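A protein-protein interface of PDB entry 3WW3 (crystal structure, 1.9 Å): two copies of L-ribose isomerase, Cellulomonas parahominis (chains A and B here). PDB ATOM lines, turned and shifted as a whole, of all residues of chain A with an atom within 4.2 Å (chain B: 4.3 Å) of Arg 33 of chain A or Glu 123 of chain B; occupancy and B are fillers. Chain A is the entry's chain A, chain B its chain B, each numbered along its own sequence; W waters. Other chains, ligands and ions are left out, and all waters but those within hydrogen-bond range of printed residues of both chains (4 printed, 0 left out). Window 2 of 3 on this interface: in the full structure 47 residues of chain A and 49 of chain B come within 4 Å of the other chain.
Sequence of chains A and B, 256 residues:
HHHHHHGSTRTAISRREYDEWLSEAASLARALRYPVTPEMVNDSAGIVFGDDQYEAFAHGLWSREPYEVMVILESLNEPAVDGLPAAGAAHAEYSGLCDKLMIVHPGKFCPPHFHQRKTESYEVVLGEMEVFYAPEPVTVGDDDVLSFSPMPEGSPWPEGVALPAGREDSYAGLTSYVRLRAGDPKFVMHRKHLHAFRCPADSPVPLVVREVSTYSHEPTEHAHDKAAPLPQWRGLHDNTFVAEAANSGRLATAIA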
ATOM      1  N   ALA A  29      -1.898   0.892  18.149  1.00  0.00           N
ATOM      2  CA  ALA A  29      -2.194  -0.312  17.373  1.00  0.00           C
ATOM      3  C   ALA A  29      -3.054   0.044  16.163  1.00  0.00           C
ATOM      4  O   ALA A  29      -2.787  -0.395  15.040  1.00  0.00           O
ATOM      5  CB  ALA A  29      -2.915  -1.336  18.250  1.00  0.00           C
ATOM      6  N   ARG A  30      -4.082   0.854  16.398  1.00  0.00           N
ATOM      7  CA  ARG A  30      -4.987   1.282  15.339  1.00  0.00           C
ATOM      8  C   ARG A  30      -4.247   2.117  14.297  1.00  0.00           C
ATOM      9  O   ARG A  30      -4.471   1.963  13.097  1.00  0.00           O
ATOM     10  CB  ARG A  30      -6.144   2.095  15.929  1.00  0.00           C
ATOM     11  CG  ARG A  30      -7.111   1.294  16.806  1.00  0.00           C
ATOM     12  CD  ARG A  30      -8.053   2.234  17.554  1.00  0.00           C
ATOM     13  NE  ARG A  30      -9.032   1.532  18.384  1.00  0.00           N
ATOM     14  CZ  ARG A  30     -10.182   1.042  17.931  1.00  0.00           C
ATOM     15  NH1 ARG A  30     -10.506   1.175  16.650  1.00  0.00           N
ATOM     16  NH2 ARG A  30     -11.012   0.425  18.760  1.00  0.00           N
ATOM     17  N   ALA A  31      -3.369   3.004  14.756  1.00  0.00           N
ATOM     18  CA  ALA A  31      -2.608   3.847  13.840  1.00  0.00           C
ATOM     19  C   ALA A  31      -1.719   2.977  12.959  1.00  0.00           C
ATOM     20  O   ALA A  31      -1.412   3.339  11.821  1.00  0.00           O
ATOM     21  CB  ALA A  31      -1.758   4.848  14.621  1.00  0.00           C
ATOM     22  N   LEU A  32      -1.309   1.828  13.488  1.00  0.00           N
ATOM     23  CA  LEU A  32      -0.456   0.906  12.745  1.00  0.00           C
ATOM     24  C   LEU A  32      -1.276  -0.111  11.951  1.00  0.00           C
ATOM     25  O   LEU A  32      -0.738  -1.101  11.448  1.00  0.00           O
ATOM     26  CB  LEU A  32       0.510   0.201  13.709  1.00  0.00           C
ATOM     27  CG  LEU A  32       1.489   1.169  14.394  1.00  0.00           C
ATOM     28  CD1 LEU A  32       2.212   0.474  15.543  1.00  0.00           C
ATOM     29  CD2 LEU A  32       2.502   1.694  13.369  1.00  0.00           C
ATOM     30  N   ARG A  33      -2.576   0.153  11.846  1.00  0.00           N
ATOM     31  CA  ARG A  33      -3.523  -0.679  11.103  1.00  0.00           C
ATOM     32  C   ARG A  33      -3.845  -2.062  11.672  1.00  0.00           C
ATOM     33  O   ARG A  33      -4.271  -2.947  10.930  1.00  0.00           O
ATOM     34  CB  ARG A  33      -3.060  -0.830   9.647  1.00  0.00           C
ATOM     35  CG  ARG A  33      -2.990   0.490   8.875  1.00  0.00           C
ATOM     36  CD  ARG A  33      -2.488   0.280   7.446  1.00  0.00           C
ATOM     37  NE  ARG A  33      -2.374   1.537   6.705  1.00  0.00           N
ATOM     38  CZ  ARG A  33      -3.409   2.259   6.288  1.00  0.00           C
ATOM     39  NH1 ARG A  33      -4.648   1.853   6.531  1.00  0.00           N
ATOM     40  NH2 ARG A  33      -3.206   3.390   5.630  1.00  0.00           N
ATOM     41  N   TYR A  34      -3.638  -2.265  12.972  1.00  0.00           N
ATOM     42  CA  TYR A  34      -3.964  -3.556  13.577  1.00  0.00           C
ATOM     43  C   TYR A  34      -5.458  -3.498  13.909  1.00  0.00           C
ATOM     44  O   TYR A  34      -5.938  -2.492  14.416  1.00  0.00           O
ATOM     45  CB  TYR A  34      -3.152  -3.792  14.858  1.00  0.00           C
ATOM     46  CG  TYR A  34      -3.169  -5.242  15.296  1.00  0.00           C
ATOM     47  CD1 TYR A  34      -2.443  -6.207  14.596  1.00  0.00           C
ATOM     48  CD2 TYR A  34      -3.937  -5.657  16.381  1.00  0.00           C
ATOM     49  CE1 TYR A  34      -2.480  -7.547  14.961  1.00  0.00           C
ATOM     50  CE2 TYR A  34      -3.985  -7.001  16.759  1.00  0.00           C
ATOM     51  CZ  TYR A  34      -3.255  -7.941  16.045  1.00  0.00           C
ATOM     52  OH  TYR A  34      -3.290  -9.268  16.411  1.00  0.00           O
ATOM     53  N   PRO A  35      -6.212  -4.576  13.625  1.00  0.00           N
ATOM     54  CA  PRO A  35      -7.652  -4.591  13.905  1.00  0.00           C
ATOM     55  C   PRO A  35      -8.013  -4.728  15.381  1.00  0.00           C
ATOM     56  O   PRO A  35      -8.012  -5.825  15.932  1.00  0.00           O
ATOM     57  CB  PRO A  35      -8.145  -5.765  13.070  1.00  0.00           C
ATOM     58  CG  PRO A  35      -7.004  -6.729  13.174  1.00  0.00           C
ATOM     59  CD  PRO A  35      -5.790  -5.832  12.978  1.00  0.00           C
ATOM     60  N   ARG A 210       3.967  -7.816  15.865  1.00  0.00           N
ATOM     61  CA  ARG A 210       2.836  -8.681  15.571  1.00  0.00           C
ATOM     62  C   ARG A 210       3.318 -10.113  15.719  1.00  0.00           C
ATOM     63  O   ARG A 210       4.314 -10.520  15.111  1.00  0.00           O
ATOM     64  CB  ARG A 210       2.306  -8.484  14.145  1.00  0.00           C
ATOM     65  CG  ARG A 210       1.129  -9.426  13.825  1.00  0.00           C
ATOM     66  CD  ARG A 210       0.706  -9.380  12.355  1.00  0.00           C
ATOM     67  NE  ARG A 210       0.175  -8.080  11.953  1.00  0.00           N
ATOM     68  CZ  ARG A 210      -1.107  -7.832  11.698  1.00  0.00           C
ATOM     69  NH1 ARG A 210      -1.488  -6.614  11.335  1.00  0.00           N
ATOM     70  NH2 ARG A 210      -2.009  -8.796  11.808  1.00  0.00           N
ATOM     71  N   LEU B  32       1.943  -0.205   3.285  1.00  0.00           N
ATOM     72  CA  LEU B  32       0.991  -0.666   4.290  1.00  0.00           C
ATOM     73  C   LEU B  32       1.674  -1.395   5.451  1.00  0.00           C
ATOM     74  O   LEU B  32       1.009  -2.011   6.286  1.00  0.00           O
ATOM     75  CB  LEU B  32      -0.061  -1.576   3.638  1.00  0.00           C
ATOM     76  CG  LEU B  32      -0.951  -0.887   2.590  1.00  0.00           C
ATOM     77  CD1 LEU B  32      -1.714  -1.926   1.782  1.00  0.00           C
ATOM     78  CD2 LEU B  32      -1.918   0.064   3.273  1.00  0.00           C
ATOM     79  N   TYR B 122      -8.788 -14.031   7.631  1.00  0.00           N
ATOM     80  CA  TYR B 122      -8.573 -12.845   6.812  1.00  0.00           C
ATOM     81  C   TYR B 122      -8.604 -11.543   7.601  1.00  0.00           C
ATOM     82  O   TYR B 122      -9.412 -11.370   8.513  1.00  0.00           O
ATOM     83  CB  TYR B 122      -9.638 -12.735   5.717  1.00  0.00           C
ATOM     84  CG  TYR B 122      -9.913 -14.002   4.956  1.00  0.00           C
ATOM     85  CD1 TYR B 122      -8.875 -14.749   4.402  1.00  0.00           C
ATOM     86  CD2 TYR B 122     -11.221 -14.443   4.766  1.00  0.00           C
ATOM     87  CE1 TYR B 122      -9.136 -15.910   3.675  1.00  0.00           C
ATOM     88  CE2 TYR B 122     -11.493 -15.599   4.042  1.00  0.00           C
ATOM     89  CZ  TYR B 122     -10.449 -16.328   3.501  1.00  0.00           C
ATOM     90  OH  TYR B 122     -10.724 -17.475   2.792  1.00  0.00           O
ATOM     91  N   GLU B 123      -7.726 -10.627   7.215  1.00  0.00           N
ATOM     92  CA  GLU B 123      -7.643  -9.306   7.822  1.00  0.00           C
ATOM     93  C   GLU B 123      -7.471  -8.325   6.672  1.00  0.00           C
ATOM     94  O   GLU B 123      -6.387  -8.237   6.090  1.00  0.00           O
ATOM     95  CB  GLU B 123      -6.430  -9.202   8.752  1.00  0.00           C
ATOM     96  CG  GLU B 123      -6.274  -7.817   9.384  1.00  0.00           C
ATOM     97  CD  GLU B 123      -4.905  -7.605  10.017  1.00  0.00           C
ATOM     98  OE1 GLU B 123      -4.391  -8.545  10.648  1.00  0.00           O
ATOM     99  OE2 GLU B 123      -4.349  -6.493   9.891  1.00  0.00           O
ATOM    100  N   VAL B 124      -8.533  -7.600   6.330  1.00  0.00           N
ATOM    101  CA  VAL B 124      -8.445  -6.636   5.242  1.00  0.00           C
ATOM    102  C   VAL B 124      -7.568  -5.460   5.662  1.00  0.00           C
ATOM    103  O   VAL B 124      -7.761  -4.879   6.734  1.00  0.00           O
ATOM    104  CB  VAL B 124      -9.836  -6.115   4.841  1.00  0.00           C
ATOM    105  CG1 VAL B 124      -9.696  -5.027   3.795  1.00  0.00           C
ATOM    106  CG2 VAL B 124     -10.688  -7.264   4.307  1.00  0.00           C
ATOM    107  N   VAL B 125      -6.600  -5.113   4.823  1.00  0.00           N
ATOM    108  CA  VAL B 125      -5.695  -4.009   5.119  1.00  0.00           C
ATOM    109  C   VAL B 125      -6.118  -2.758   4.358  1.00  0.00           C
ATOM    110  O   VAL B 125      -6.086  -1.652   4.896  1.00  0.00           O
ATOM    111  CB  VAL B 125      -4.243  -4.352   4.726  1.00  0.00           C
ATOM    112  CG1 VAL B 125      -3.310  -3.203   5.109  1.00  0.00           C
ATOM    113  CG2 VAL B 125      -3.818  -5.644   5.402  1.00  0.00           C
ATOM    114  N   LYS B 186     -11.218 -10.467  12.850  1.00  0.00           N
ATOM    115  CA  LYS B 186     -10.631 -11.480  11.979  1.00  0.00           C
ATOM    116  C   LYS B 186     -11.739 -12.419  11.493  1.00  0.00           C
ATOM    117  O   LYS B 186     -12.653 -12.730  12.250  1.00  0.00           O
ATOM    118  CB  LYS B 186      -9.604 -12.300  12.762  1.00  0.00           C
ATOM    119  CG  LYS B 186      -8.329 -11.565  13.138  1.00  0.00           C
ATOM    120  CD  LYS B 186      -7.365 -11.516  11.961  1.00  0.00           C
ATOM    121  CE  LYS B 186      -5.967 -11.143  12.408  1.00  0.00           C
ATOM    122  NZ  LYS B 186      -4.973 -11.185  11.286  1.00  0.00           N
ATOM    123  N   VAL B 209      -5.183  -7.871   1.492  1.00  0.00           N
ATOM    124  CA  VAL B 209      -5.594  -8.658   2.642  1.00  0.00           C
ATOM    125  C   VAL B 209      -4.492  -9.530   3.218  1.00  0.00           C
ATOM    126  O   VAL B 209      -3.750 -10.190   2.488  1.00  0.00           O
ATOM    127  CB  VAL B 209      -6.799  -9.560   2.285  1.00  0.00           C
ATOM    128  CG1 VAL B 209      -6.495 -10.352   1.034  1.00  0.00           C
ATOM    129  CG2 VAL B 209      -7.112 -10.514   3.442  1.00  0.00           C
ATOM    130  N   ARG B 210      -4.382  -9.519   4.539  1.00  0.00           N
ATOM    131  CA  ARG B 210      -3.388 -10.339   5.199  1.00  0.00           C
ATOM    132  C   ARG B 210      -4.061 -11.639   5.586  1.00  0.00           C
ATOM    133  O   ARG B 210      -5.080 -11.646   6.280  1.00  0.00           O
ATOM    134  CB  ARG B 210      -2.842  -9.668   6.461  1.00  0.00           C
ATOM    135  CG  ARG B 210      -1.771 -10.516   7.153  1.00  0.00           C
ATOM    136  CD  ARG B 210      -1.397  -9.967   8.522  1.00  0.00           C
ATOM    137  NE  ARG B 210      -0.710  -8.679   8.457  1.00  0.00           N
ATOM    138  CZ  ARG B 210       0.601  -8.517   8.621  1.00  0.00           C
ATOM    139  NH1 ARG B 210       1.136  -7.306   8.549  1.00  0.00           N
ATOM    140  NH2 ARG B 210       1.376  -9.566   8.861  1.00  0.00           N
HETATM  141  O   HOH W   1       1.179  -5.808  11.510  1.00  0.00           O
HETATM  142  O   HOH W   2      -3.556  -4.456   8.628  1.00  0.00           O
HETATM  143  O   HOH W   3      -5.959  -0.927   7.557  1.00  0.00           O
HETATM  144  O   HOH W   4      -1.222  -6.268   8.038  1.00  0.00           O
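Water W4 bridges NE of Arg 210 of chain B (2.5 Å) and NH1 of Arg 210 of chain A (3.3 Å). Water W1 lies within hydrogen-bond range of the guanidinium group (NE) of Arg 210 of chain A (2.5 Å) and the guanidinium group (NH1) of Arg 210 of chain B (3.3 Å). Water W2 lies within hydrogen-bond range of OE2 of Glu 123 of chain B (2.5 Å) and O of Arg 33 of chain A (2.8 Å). Water W3 lies within hydrogen-bond range of O of Val 125 of chain B and NH1 of Arg 33 of chain A.
Arg 30 of chain A touches none of the printed residues of chain B. Leu 32 of chain A touches none of the printed residues of chain B. Of the printed residues of chain B, Pro 35 of chain A touches Glu 123 (3.5 Å). Printed residues of chain B within 4 Å of Arg 210 of chain A: Glu 123 (2.7 Å), Lys 186 (3.8 Å) and Arg 210 (3.4 Å). Printed residues of chain A within 4 Å of Leu 32 of chain B: Arg 33. The nearest residue of chain B that does not touch Arg 33 of chain A is Val 125 of chain B (4.1 Å). The nearest printed residue of chain A that does not touch Lys 186 of chain B is Pro 35 of chain A (4.6 Å).
Of the 8 printed residues of chain B, 4 touch a printed residue of chain A. Hydrophobic or aromatic side chains of chain B that line the printed part of chain A: Leu 32. Among the printed residues, Asp or Glu carboxylates within 4 Å of a Lys or Arg side-chain nitrogen of the other chain: Arg 210 of chain A with Glu 123 of chain B.
Arg 210 of chain B touches its own counterpart, Arg 210 of chain A. Positions printed for both chains: 32 and 210. Of the 6 pairs that touch across the chains among the printed residues, 1 has its exchanged pair printed and touching as well.
The backbone NH (N) of Arg 210 of chain B sits at hydrogen-bond distance from the backbone carbonyl oxygen (O) of Glu 123 of chain B (2.8 Å). The side-chain carboxylate (OE1) of Glu 123 of chain B is in salt-bridge range of the side-chain amino group (NZ) of Lys 186 of chain B, at 2.8 Å.
NE of Arg 33 of chain A touches CD2 of Leu 32 of chain B, at 3.8 Å. Glu 123 of chain B touches Arg 33 of chain A (OE2 to O, 3.7 Å). CD of Pro 35 of chain A touches OE2 of Glu 123 of chain B, at 3.5 Å. Lys 186 of chain B touches Arg 210 of chain A (NZ to NH2, 3.8 Å). NE of Arg 210 of chain B touches CZ of Arg 210 of chain A, 3.4 Å away.
The guanidinium group (NH2) of Arg 210 of chain A lies within salt-bridge range of the side-chain carboxylate (OE1) of Glu 123 of chain B.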
